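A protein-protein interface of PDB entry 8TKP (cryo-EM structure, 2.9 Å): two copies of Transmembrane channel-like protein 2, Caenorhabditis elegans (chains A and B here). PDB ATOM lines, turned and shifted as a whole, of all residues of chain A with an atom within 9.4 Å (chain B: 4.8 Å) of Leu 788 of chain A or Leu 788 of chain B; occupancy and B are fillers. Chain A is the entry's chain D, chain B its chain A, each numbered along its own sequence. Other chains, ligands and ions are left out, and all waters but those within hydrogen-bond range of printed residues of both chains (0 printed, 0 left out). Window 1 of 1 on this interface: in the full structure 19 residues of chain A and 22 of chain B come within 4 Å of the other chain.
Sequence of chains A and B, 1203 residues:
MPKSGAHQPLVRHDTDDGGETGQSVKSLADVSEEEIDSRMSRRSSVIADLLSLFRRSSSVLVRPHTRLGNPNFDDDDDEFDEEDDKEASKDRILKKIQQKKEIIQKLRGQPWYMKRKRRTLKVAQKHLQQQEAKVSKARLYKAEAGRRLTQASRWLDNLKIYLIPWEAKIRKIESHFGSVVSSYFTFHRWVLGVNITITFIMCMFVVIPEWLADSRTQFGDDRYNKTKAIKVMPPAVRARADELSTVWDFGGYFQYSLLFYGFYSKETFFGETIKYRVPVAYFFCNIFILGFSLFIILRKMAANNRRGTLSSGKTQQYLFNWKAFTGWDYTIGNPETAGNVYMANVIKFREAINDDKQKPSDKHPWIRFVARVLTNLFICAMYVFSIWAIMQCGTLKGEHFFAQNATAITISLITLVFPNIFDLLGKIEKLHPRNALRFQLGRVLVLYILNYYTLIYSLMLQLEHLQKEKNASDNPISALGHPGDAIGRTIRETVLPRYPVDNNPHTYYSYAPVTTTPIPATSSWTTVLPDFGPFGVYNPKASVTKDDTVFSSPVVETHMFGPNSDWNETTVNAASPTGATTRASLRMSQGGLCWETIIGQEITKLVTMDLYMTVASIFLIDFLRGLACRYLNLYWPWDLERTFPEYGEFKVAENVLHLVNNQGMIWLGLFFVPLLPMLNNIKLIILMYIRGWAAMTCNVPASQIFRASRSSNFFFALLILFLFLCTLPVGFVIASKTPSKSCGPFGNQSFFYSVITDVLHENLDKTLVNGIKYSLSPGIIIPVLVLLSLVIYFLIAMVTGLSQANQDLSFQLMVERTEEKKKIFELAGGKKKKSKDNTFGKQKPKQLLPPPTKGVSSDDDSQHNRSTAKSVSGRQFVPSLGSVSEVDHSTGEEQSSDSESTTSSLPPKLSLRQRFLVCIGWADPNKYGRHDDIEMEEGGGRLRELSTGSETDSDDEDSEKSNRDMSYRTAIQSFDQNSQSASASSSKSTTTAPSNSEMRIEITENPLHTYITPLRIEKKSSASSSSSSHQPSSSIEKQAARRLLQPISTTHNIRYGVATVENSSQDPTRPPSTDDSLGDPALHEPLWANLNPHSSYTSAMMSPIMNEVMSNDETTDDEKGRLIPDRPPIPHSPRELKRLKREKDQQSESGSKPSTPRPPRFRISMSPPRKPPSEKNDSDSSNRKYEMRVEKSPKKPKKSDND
The backbone carbonyl oxygen (O) of Leu 785 of chain A sits at hydrogen-bond distance from the side-chain hydroxyl (OG) of Ser 789 of chain A (3.3 Å).
Among the printed residues, pairs that only touch across the chains: Leu 294 of chain A with Leu 790 of chain B, Val 784 of chain A with Leu 785 of chain B, Leu 785 of chain A with Val 784 of chain B, Leu 785 of chain A with Leu 788 of chain B, Leu 788 of chain A with Leu 788 of chain B, Leu 788 of chain A with Ile 792 of chain B, Ile 792 of chain A with Leu 788 of chain B and Ile 792 of chain A with Ile 792 of chain B.
Of the printed residues of chain B, Val 784 of chain A touches Leu 785. Printed residues of chain B within 4 Å of Leu 785 of chain A: Val 784 and Leu 788. Leu 788 of chain A touches just these residues of chain B: Leu 788 and Ile 792. Ser 789 of chain A touches none of the printed residues of chain B. Printed residues of chain A within 4 Å of Leu 785 of chain B: Val 784 (3.9 Å). Leu 788 of chain B touches just these residues of chain A: Leu 785, Leu 788 and Ile 792. Ser 789 of chain B touches none of the printed residues of chain A. Of the printed residues of chain A, Leu 790 of chain B touches Leu 294. Printed residues of chain A within 4 Å of Ile 792 of chain B: Leu 788 and Ile 792. The nearest printed residue of chain B that does not touch Leu 788 of chain A is Ser 789 of chain B (5.1 Å).
Printed residues of chain A that touch a printed residue of chain B: Leu 294, Val 784, Leu 785, Leu 788 and Ile 792. Hydrophobic or aromatic side chains of chain A within 4 Å of the printed part of chain B: Leu 294, Val 784, Leu 785, Leu 788 and Ile 792. Of the 9 printed residues of chain B, 5 touch a printed residue of chain A. Printed residues of chain B that touch a printed residue of chain A: Val 784, Leu 785, Leu 788, Leu 790 and Ile 792. Hydrophobic or aromatic side chains of chain B that line the printed part of chain A: Val 784, Leu 785, Leu 788, Leu 790 and Ile 792. Among the printed residues, 8 pairs touch across the chains.
Val 784 of chain A touches Leu 785 of chain B, and with the chains exchanged Leu 785 of chain A touches Val 784 of chain B. Leu 785 of chain A touches Leu 788 of chain B, but with the chains exchanged Leu 788 of chain A does not touch Leu 785 of chain B (5.2 Å). Leu 788 of chain A touches its own counterpart, Leu 788 of chain B. Leu 788 of chain A touches Ile 792 of chain B, and with the chains exchanged Ile 792 of chain A touches Leu 788 of chain B. Of the 8 pairs that touch across the chains among the printed residues, 6 have their exchanged pair printed and touching as well.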
ATOM      1  N   LEU A 294      27.719  12.330  20.259  1.00  0.00           N
ATOM      2  CA  LEU A 294      27.747  10.874  20.163  1.00  0.00           C
ATOM      3  C   LEU A 294      27.531  10.423  18.724  1.00  0.00           C
ATOM      4  O   LEU A 294      28.259   9.563  18.211  1.00  0.00           O
ATOM      5  CB  LEU A 294      26.688  10.265  21.083  1.00  0.00           C
ATOM      6  CG  LEU A 294      26.755   8.750  21.263  1.00  0.00           C
ATOM      7  CD1 LEU A 294      28.054   8.367  21.949  1.00  0.00           C
ATOM      8  CD2 LEU A 294      25.557   8.239  22.052  1.00  0.00           C
ATOM      9  N   PHE A 724      30.930   9.271  27.430  1.00  0.00           N
ATOM     10  CA  PHE A 724      30.036   8.580  28.356  1.00  0.00           C
ATOM     11  C   PHE A 724      30.356   8.941  29.803  1.00  0.00           C
ATOM     12  O   PHE A 724      29.454   9.249  30.600  1.00  0.00           O
ATOM     13  CB  PHE A 724      30.133   7.070  28.137  1.00  0.00           C
ATOM     14  CG  PHE A 724      29.628   6.257  29.291  1.00  0.00           C
ATOM     15  CD1 PHE A 724      28.271   6.155  29.544  1.00  0.00           C
ATOM     16  CD2 PHE A 724      30.511   5.586  30.121  1.00  0.00           C
ATOM     17  CE1 PHE A 724      27.805   5.405  30.606  1.00  0.00           C
ATOM     18  CE2 PHE A 724      30.051   4.834  31.183  1.00  0.00           C
ATOM     19  CZ  PHE A 724      28.696   4.742  31.426  1.00  0.00           C
ATOM     20  N   ILE A 781      12.545   0.212  32.623  1.00  0.00           N
ATOM     21  CA  ILE A 781      13.897   0.256  32.070  1.00  0.00           C
ATOM     22  C   ILE A 781      14.741  -0.918  32.554  1.00  0.00           C
ATOM     23  O   ILE A 781      15.567  -1.445  31.809  1.00  0.00           O
ATOM     24  CB  ILE A 781      14.565   1.606  32.410  1.00  0.00           C
ATOM     25  CG1 ILE A 781      13.604   2.762  32.124  1.00  0.00           C
ATOM     26  CG2 ILE A 781      15.848   1.782  31.614  1.00  0.00           C
ATOM     27  CD1 ILE A 781      14.163   4.123  32.476  1.00  0.00           C
ATOM     28  N   ILE A 782      14.551  -1.333  33.804  1.00  0.00           N
ATOM     29  CA  ILE A 782      15.351  -2.389  34.424  1.00  0.00           C
ATOM     30  C   ILE A 782      15.253  -3.710  33.660  1.00  0.00           C
ATOM     31  O   ILE A 782      16.296  -4.338  33.413  1.00  0.00           O
ATOM     32  CB  ILE A 782      14.961  -2.577  35.901  1.00  0.00           C
ATOM     33  CG1 ILE A 782      15.304  -1.319  36.702  1.00  0.00           C
ATOM     34  CG2 ILE A 782      15.658  -3.794  36.493  1.00  0.00           C
ATOM     35  CD1 ILE A 782      14.982  -1.426  38.176  1.00  0.00           C
ATOM     36  N   PRO A 783      14.058  -4.193  33.280  1.00  0.00           N
ATOM     37  CA  PRO A 783      14.019  -5.437  32.489  1.00  0.00           C
ATOM     38  C   PRO A 783      14.779  -5.336  31.179  1.00  0.00           C
ATOM     39  O   PRO A 783      15.414  -6.310  30.756  1.00  0.00           O
ATOM     40  CB  PRO A 783      12.517  -5.666  32.266  1.00  0.00           C
ATOM     41  CG  PRO A 783      11.887  -4.336  32.473  1.00  0.00           C
ATOM     42  CD  PRO A 783      12.696  -3.697  33.553  1.00  0.00           C
ATOM     43  N   VAL A 784      14.739  -4.170  30.530  1.00  0.00           N
ATOM     44  CA  VAL A 784      15.502  -3.974  29.299  1.00  0.00           C
ATOM     45  C   VAL A 784      16.993  -4.099  29.582  1.00  0.00           C
ATOM     46  O   VAL A 784      17.739  -4.719  28.815  1.00  0.00           O
ATOM     47  CB  VAL A 784      15.157  -2.615  28.665  1.00  0.00           C
ATOM     48  CG1 VAL A 784      15.915  -2.429  27.358  1.00  0.00           C
ATOM     49  CG2 VAL A 784      13.657  -2.500  28.440  1.00  0.00           C
ATOM     50  N   LEU A 785      17.450  -3.507  30.688  1.00  0.00           N
ATOM     51  CA  LEU A 785      18.862  -3.587  31.050  1.00  0.00           C
ATOM     52  C   LEU A 785      19.277  -5.030  31.325  1.00  0.00           C
ATOM     53  O   LEU A 785      20.355  -5.468  30.908  1.00  0.00           O
ATOM     54  CB  LEU A 785      19.138  -2.696  32.263  1.00  0.00           C
ATOM     55  CG  LEU A 785      20.590  -2.397  32.655  1.00  0.00           C
ATOM     56  CD1 LEU A 785      21.156  -3.453  33.598  1.00  0.00           C
ATOM     57  CD2 LEU A 785      21.465  -2.256  31.416  1.00  0.00           C
ATOM     58  N   VAL A 786      18.431  -5.783  32.034  1.00  0.00           N
ATOM     59  CA  VAL A 786      18.747  -7.178  32.330  1.00  0.00           C
ATOM     60  C   VAL A 786      18.821  -7.993  31.045  1.00  0.00           C
ATOM     61  O   VAL A 786      19.734  -8.810  30.850  1.00  0.00           O
ATOM     62  CB  VAL A 786      17.718  -7.768  33.313  1.00  0.00           C
ATOM     63  CG1 VAL A 786      18.007  -9.240  33.561  1.00  0.00           C
ATOM     64  CG2 VAL A 786      17.726  -6.991  34.619  1.00  0.00           C
ATOM     65  N   LEU A 787      17.853  -7.787  30.147  1.00  0.00           N
ATOM     66  CA  LEU A 787      17.858  -8.499  28.875  1.00  0.00           C
ATOM     67  C   LEU A 787      19.106  -8.163  28.069  1.00  0.00           C
ATOM     68  O   LEU A 787      19.731  -9.048  27.476  1.00  0.00           O
ATOM     69  CB  LEU A 787      16.589  -8.167  28.086  1.00  0.00           C
ATOM     70  CG  LEU A 787      16.363  -8.868  26.743  1.00  0.00           C
ATOM     71  CD1 LEU A 787      14.893  -9.214  26.571  1.00  0.00           C
ATOM     72  CD2 LEU A 787      16.837  -8.002  25.584  1.00  0.00           C
ATOM     73  N   LEU A 788      19.485  -6.883  28.042  1.00  0.00           N
ATOM     74  CA  LEU A 788      20.682  -6.474  27.319  1.00  0.00           C
ATOM     75  C   LEU A 788      21.929  -7.122  27.908  1.00  0.00           C
ATOM     76  O   LEU A 788      22.802  -7.597  27.174  1.00  0.00           O
ATOM     77  CB  LEU A 788      20.807  -4.948  27.330  1.00  0.00           C
ATOM     78  CG  LEU A 788      20.327  -4.208  26.078  1.00  0.00           C
ATOM     79  CD1 LEU A 788      21.175  -4.593  24.877  1.00  0.00           C
ATOM     80  CD2 LEU A 788      18.856  -4.476  25.804  1.00  0.00           C
ATOM     81  N   SER A 789      22.024  -7.161  29.238  1.00  0.00           N
ATOM     82  CA  SER A 789      23.180  -7.787  29.873  1.00  0.00           C
ATOM     83  C   SER A 789      23.265  -9.268  29.525  1.00  0.00           C
ATOM     84  O   SER A 789      24.341  -9.778  29.186  1.00  0.00           O
ATOM     85  CB  SER A 789      23.117  -7.590  31.387  1.00  0.00           C
ATOM     86  OG  SER A 789      21.937  -8.161  31.926  1.00  0.00           O
ATOM     87  N   LEU A 790      22.135  -9.975  29.580  1.00  0.00           N
ATOM     88  CA  LEU A 790      22.175 -11.404  29.281  1.00  0.00           C
ATOM     89  C   LEU A 790      22.487 -11.660  27.808  1.00  0.00           C
ATOM     90  O   LEU A 790      23.247 -12.582  27.483  1.00  0.00           O
ATOM     91  CB  LEU A 790      20.865 -12.071  29.694  1.00  0.00           C
ATOM     92  CG  LEU A 790      20.879 -12.645  31.120  1.00  0.00           C
ATOM     93  CD1 LEU A 790      20.903 -11.541  32.170  1.00  0.00           C
ATOM     94  CD2 LEU A 790      19.710 -13.589  31.353  1.00  0.00           C
ATOM     95  N   VAL A 791      21.927 -10.853  26.900  1.00  0.00           N
ATOM     96  CA  VAL A 791      22.189 -11.083  25.480  1.00  0.00           C
ATOM     97  C   VAL A 791      23.634 -10.746  25.135  1.00  0.00           C
ATOM     98  O   VAL A 791      24.243 -11.398  24.281  1.00  0.00           O
ATOM     99  CB  VAL A 791      21.188 -10.318  24.588  1.00  0.00           C
ATOM    100  CG1 VAL A 791      19.757 -10.751  24.880  1.00  0.00           C
ATOM    101  CG2 VAL A 791      21.351  -8.815  24.715  1.00  0.00           C
ATOM    102  N   ILE A 792      24.217  -9.731  25.785  1.00  0.00           N
ATOM    103  CA  ILE A 792      25.624  -9.456  25.512  1.00  0.00           C
ATOM    104  C   ILE A 792      26.510 -10.539  26.115  1.00  0.00           C
ATOM    105  O   ILE A 792      27.567 -10.853  25.559  1.00  0.00           O
ATOM    106  CB  ILE A 792      26.050  -8.050  25.986  1.00  0.00           C
ATOM    107  CG1 ILE A 792      26.009  -7.930  27.509  1.00  0.00           C
ATOM    108  CG2 ILE A 792      25.203  -6.980  25.318  1.00  0.00           C
ATOM    109  CD1 ILE A 792      26.613  -6.650  28.036  1.00  0.00           C
ATOM    110  N   TYR A 793      26.109 -11.136  27.241  1.00  0.00           N
ATOM    111  CA  TYR A 793      26.854 -12.289  27.746  1.00  0.00           C
ATOM    112  C   TYR A 793      26.818 -13.446  26.751  1.00  0.00           C
ATOM    113  O   TYR A 793      27.849 -14.079  26.477  1.00  0.00           O
ATOM    114  CB  TYR A 793      26.294 -12.729  29.099  1.00  0.00           C
ATOM    115  CG  TYR A 793      26.482 -11.717  30.207  1.00  0.00           C
ATOM    116  CD1 TYR A 793      27.478 -10.752  30.132  1.00  0.00           C
ATOM    117  CD2 TYR A 793      25.663 -11.728  31.328  1.00  0.00           C
ATOM    118  CE1 TYR A 793      27.653  -9.826  31.142  1.00  0.00           C
ATOM    119  CE2 TYR A 793      25.829 -10.806  32.342  1.00  0.00           C
ATOM    120  CZ  TYR A 793      26.824  -9.858  32.245  1.00  0.00           C
ATOM    121  OH  TYR A 793      26.994  -8.937  33.254  1.00  0.00           O
ATOM    122  N   PHE A 794      25.637 -13.730  26.194  1.00  0.00           N
ATOM    123  CA  PHE A 794      25.523 -14.789  25.197  1.00  0.00           C
ATOM    124  C   PHE A 794      26.338 -14.477  23.946  1.00  0.00           C
ATOM    125  O   PHE A 794      26.991 -15.369  23.392  1.00  0.00           O
ATOM    126  CB  PHE A 794      24.056 -15.012  24.831  1.00  0.00           C
ATOM    127  N   LEU A 795      26.313 -13.221  23.492  1.00  0.00           N
ATOM    128  CA  LEU A 795      27.105 -12.826  22.334  1.00  0.00           C
ATOM    129  C   LEU A 795      28.598 -12.926  22.613  1.00  0.00           C
ATOM    130  O   LEU A 795      29.369 -13.293  21.720  1.00  0.00           O
ATOM    131  CB  LEU A 795      26.734 -11.405  21.906  1.00  0.00           C
ATOM    132  CG  LEU A 795      27.422 -10.868  20.651  1.00  0.00           C
ATOM    133  CD1 LEU A 795      27.142 -11.770  19.460  1.00  0.00           C
ATOM    134  CD2 LEU A 795      26.972  -9.444  20.365  1.00  0.00           C
ATOM    135  N   ILE A 796      29.026 -12.597  23.834  1.00  0.00           N
ATOM    136  CA  ILE A 796      30.427 -12.761  24.204  1.00  0.00           C
ATOM    137  C   ILE A 796      30.822 -14.229  24.162  1.00  0.00           C
ATOM    138  O   ILE A 796      31.901 -14.574  23.667  1.00  0.00           O
ATOM    139  CB  ILE A 796      30.690 -12.147  25.590  1.00  0.00           C
ATOM    140  N   VAL B 784      23.543   4.257  31.050  1.00  0.00           N
ATOM    141  CA  VAL B 784      23.832   2.829  30.972  1.00  0.00           C
ATOM    142  C   VAL B 784      23.093   2.194  29.800  1.00  0.00           C
ATOM    143  O   VAL B 784      23.649   1.342  29.094  1.00  0.00           O
ATOM    144  CB  VAL B 784      23.485   2.139  32.303  1.00  0.00           C
ATOM    145  CG1 VAL B 784      23.733   0.640  32.210  1.00  0.00           C
ATOM    146  CG2 VAL B 784      24.297   2.742  33.439  1.00  0.00           C
ATOM    147  N   LEU B 785      21.840   2.593  29.570  1.00  0.00           N
ATOM    148  CA  LEU B 785      21.081   2.037  28.452  1.00  0.00           C
ATOM    149  C   LEU B 785      21.710   2.403  27.112  1.00  0.00           C
ATOM    150  O   LEU B 785      21.836   1.548  26.226  1.00  0.00           O
ATOM    151  CB  LEU B 785      19.630   2.517  28.515  1.00  0.00           C
ATOM    152  CG  LEU B 785      18.684   1.956  27.452  1.00  0.00           C
ATOM    153  CD1 LEU B 785      18.617   0.439  27.538  1.00  0.00           C
ATOM    154  CD2 LEU B 785      17.297   2.566  27.592  1.00  0.00           C
ATOM    155  N   VAL B 786      22.114   3.664  26.943  1.00  0.00           N
ATOM    156  CA  VAL B 786      22.754   4.046  25.687  1.00  0.00           C
ATOM    157  C   VAL B 786      24.135   3.416  25.541  1.00  0.00           C
ATOM    158  O   VAL B 786      24.544   3.099  24.417  1.00  0.00           O
ATOM    159  CB  VAL B 786      22.827   5.577  25.530  1.00  0.00           C
ATOM    160  CG1 VAL B 786      21.440   6.190  25.673  1.00  0.00           C
ATOM    161  CG2 VAL B 786      23.795   6.195  26.519  1.00  0.00           C
ATOM    162  N   LEU B 787      24.860   3.199  26.643  1.00  0.00           N
ATOM    163  CA  LEU B 787      26.120   2.471  26.574  1.00  0.00           C
ATOM    164  C   LEU B 787      25.909   1.026  26.139  1.00  0.00           C
ATOM    165  O   LEU B 787      26.700   0.501  25.350  1.00  0.00           O
ATOM    166  CB  LEU B 787      26.833   2.525  27.927  1.00  0.00           C
ATOM    167  CG  LEU B 787      28.321   2.156  27.992  1.00  0.00           C
ATOM    168  CD1 LEU B 787      28.532   0.657  28.176  1.00  0.00           C
ATOM    169  CD2 LEU B 787      29.052   2.654  26.752  1.00  0.00           C
ATOM    170  N   LEU B 788      24.861   0.370  26.641  1.00  0.00           N
ATOM    171  CA  LEU B 788      24.522  -0.970  26.171  1.00  0.00           C
ATOM    172  C   LEU B 788      24.138  -0.974  24.696  1.00  0.00           C
ATOM    173  O   LEU B 788      24.543  -1.879  23.954  1.00  0.00           O
ATOM    174  CB  LEU B 788      23.384  -1.553  27.013  1.00  0.00           C
ATOM    175  CG  LEU B 788      23.774  -2.466  28.180  1.00  0.00           C
ATOM    176  CD1 LEU B 788      24.472  -3.714  27.666  1.00  0.00           C
ATOM    177  CD2 LEU B 788      24.648  -1.737  29.187  1.00  0.00           C
ATOM    178  N   SER B 789      23.367   0.022  24.256  1.00  0.00           N
ATOM    179  CA  SER B 789      23.019   0.120  22.843  1.00  0.00           C
ATOM    180  C   SER B 789      24.253   0.310  21.969  1.00  0.00           C
ATOM    181  O   SER B 789      24.336  -0.274  20.883  1.00  0.00           O
ATOM    182  CB  SER B 789      22.035   1.268  22.615  1.00  0.00           C
ATOM    183  OG  SER B 789      22.655   2.523  22.833  1.00  0.00           O
ATOM    184  N   LEU B 790      25.218   1.107  22.421  1.00  0.00           N
ATOM    185  CA  LEU B 790      26.464   1.276  21.685  1.00  0.00           C
ATOM    186  C   LEU B 790      27.360   0.046  21.730  1.00  0.00           C
ATOM    187  O   LEU B 790      28.067  -0.223  20.752  1.00  0.00           O
ATOM    188  CB  LEU B 790      27.239   2.482  22.223  1.00  0.00           C
ATOM    189  CG  LEU B 790      26.575   3.842  22.018  1.00  0.00           C
ATOM    190  CD1 LEU B 790      27.407   4.926  22.670  1.00  0.00           C
ATOM    191  CD2 LEU B 790      26.375   4.126  20.537  1.00  0.00           C
ATOM    192  N   VAL B 791      27.294  -0.713  22.796  1.00  0.00           N
ATOM    193  CA  VAL B 791      28.165  -1.848  22.830  1.00  0.00           C
ATOM    194  C   VAL B 791      27.548  -2.981  22.057  1.00  0.00           C
ATOM    195  O   VAL B 791      28.245  -3.700  21.355  1.00  0.00           O
ATOM    196  CB  VAL B 791      28.545  -2.257  24.251  1.00  0.00           C
ATOM    197  CG1 VAL B 791      29.366  -3.532  24.250  1.00  0.00           C
ATOM    198  CG2 VAL B 791      29.245  -1.122  24.961  1.00  0.00           C
ATOM    199  N   ILE B 792      26.229  -3.111  22.100  1.00  0.00           N
ATOM    200  CA  ILE B 792      25.630  -4.218  21.364  1.00  0.00           C
ATOM    201  C   ILE B 792      25.854  -4.105  19.874  1.00  0.00           C
ATOM    202  O   ILE B 792      26.081  -5.092  19.210  1.00  0.00           O
ATOM    203  CB  ILE B 792      24.140  -4.477  21.660  1.00  0.00           C
ATOM    204  CG1 ILE B 792      23.276  -3.268  21.349  1.00  0.00           C
ATOM    205  CG2 ILE B 792      23.952  -4.921  23.092  1.00  0.00           C
ATOM    206  CD1 ILE B 792      22.642  -3.319  19.982  1.00  0.00           C
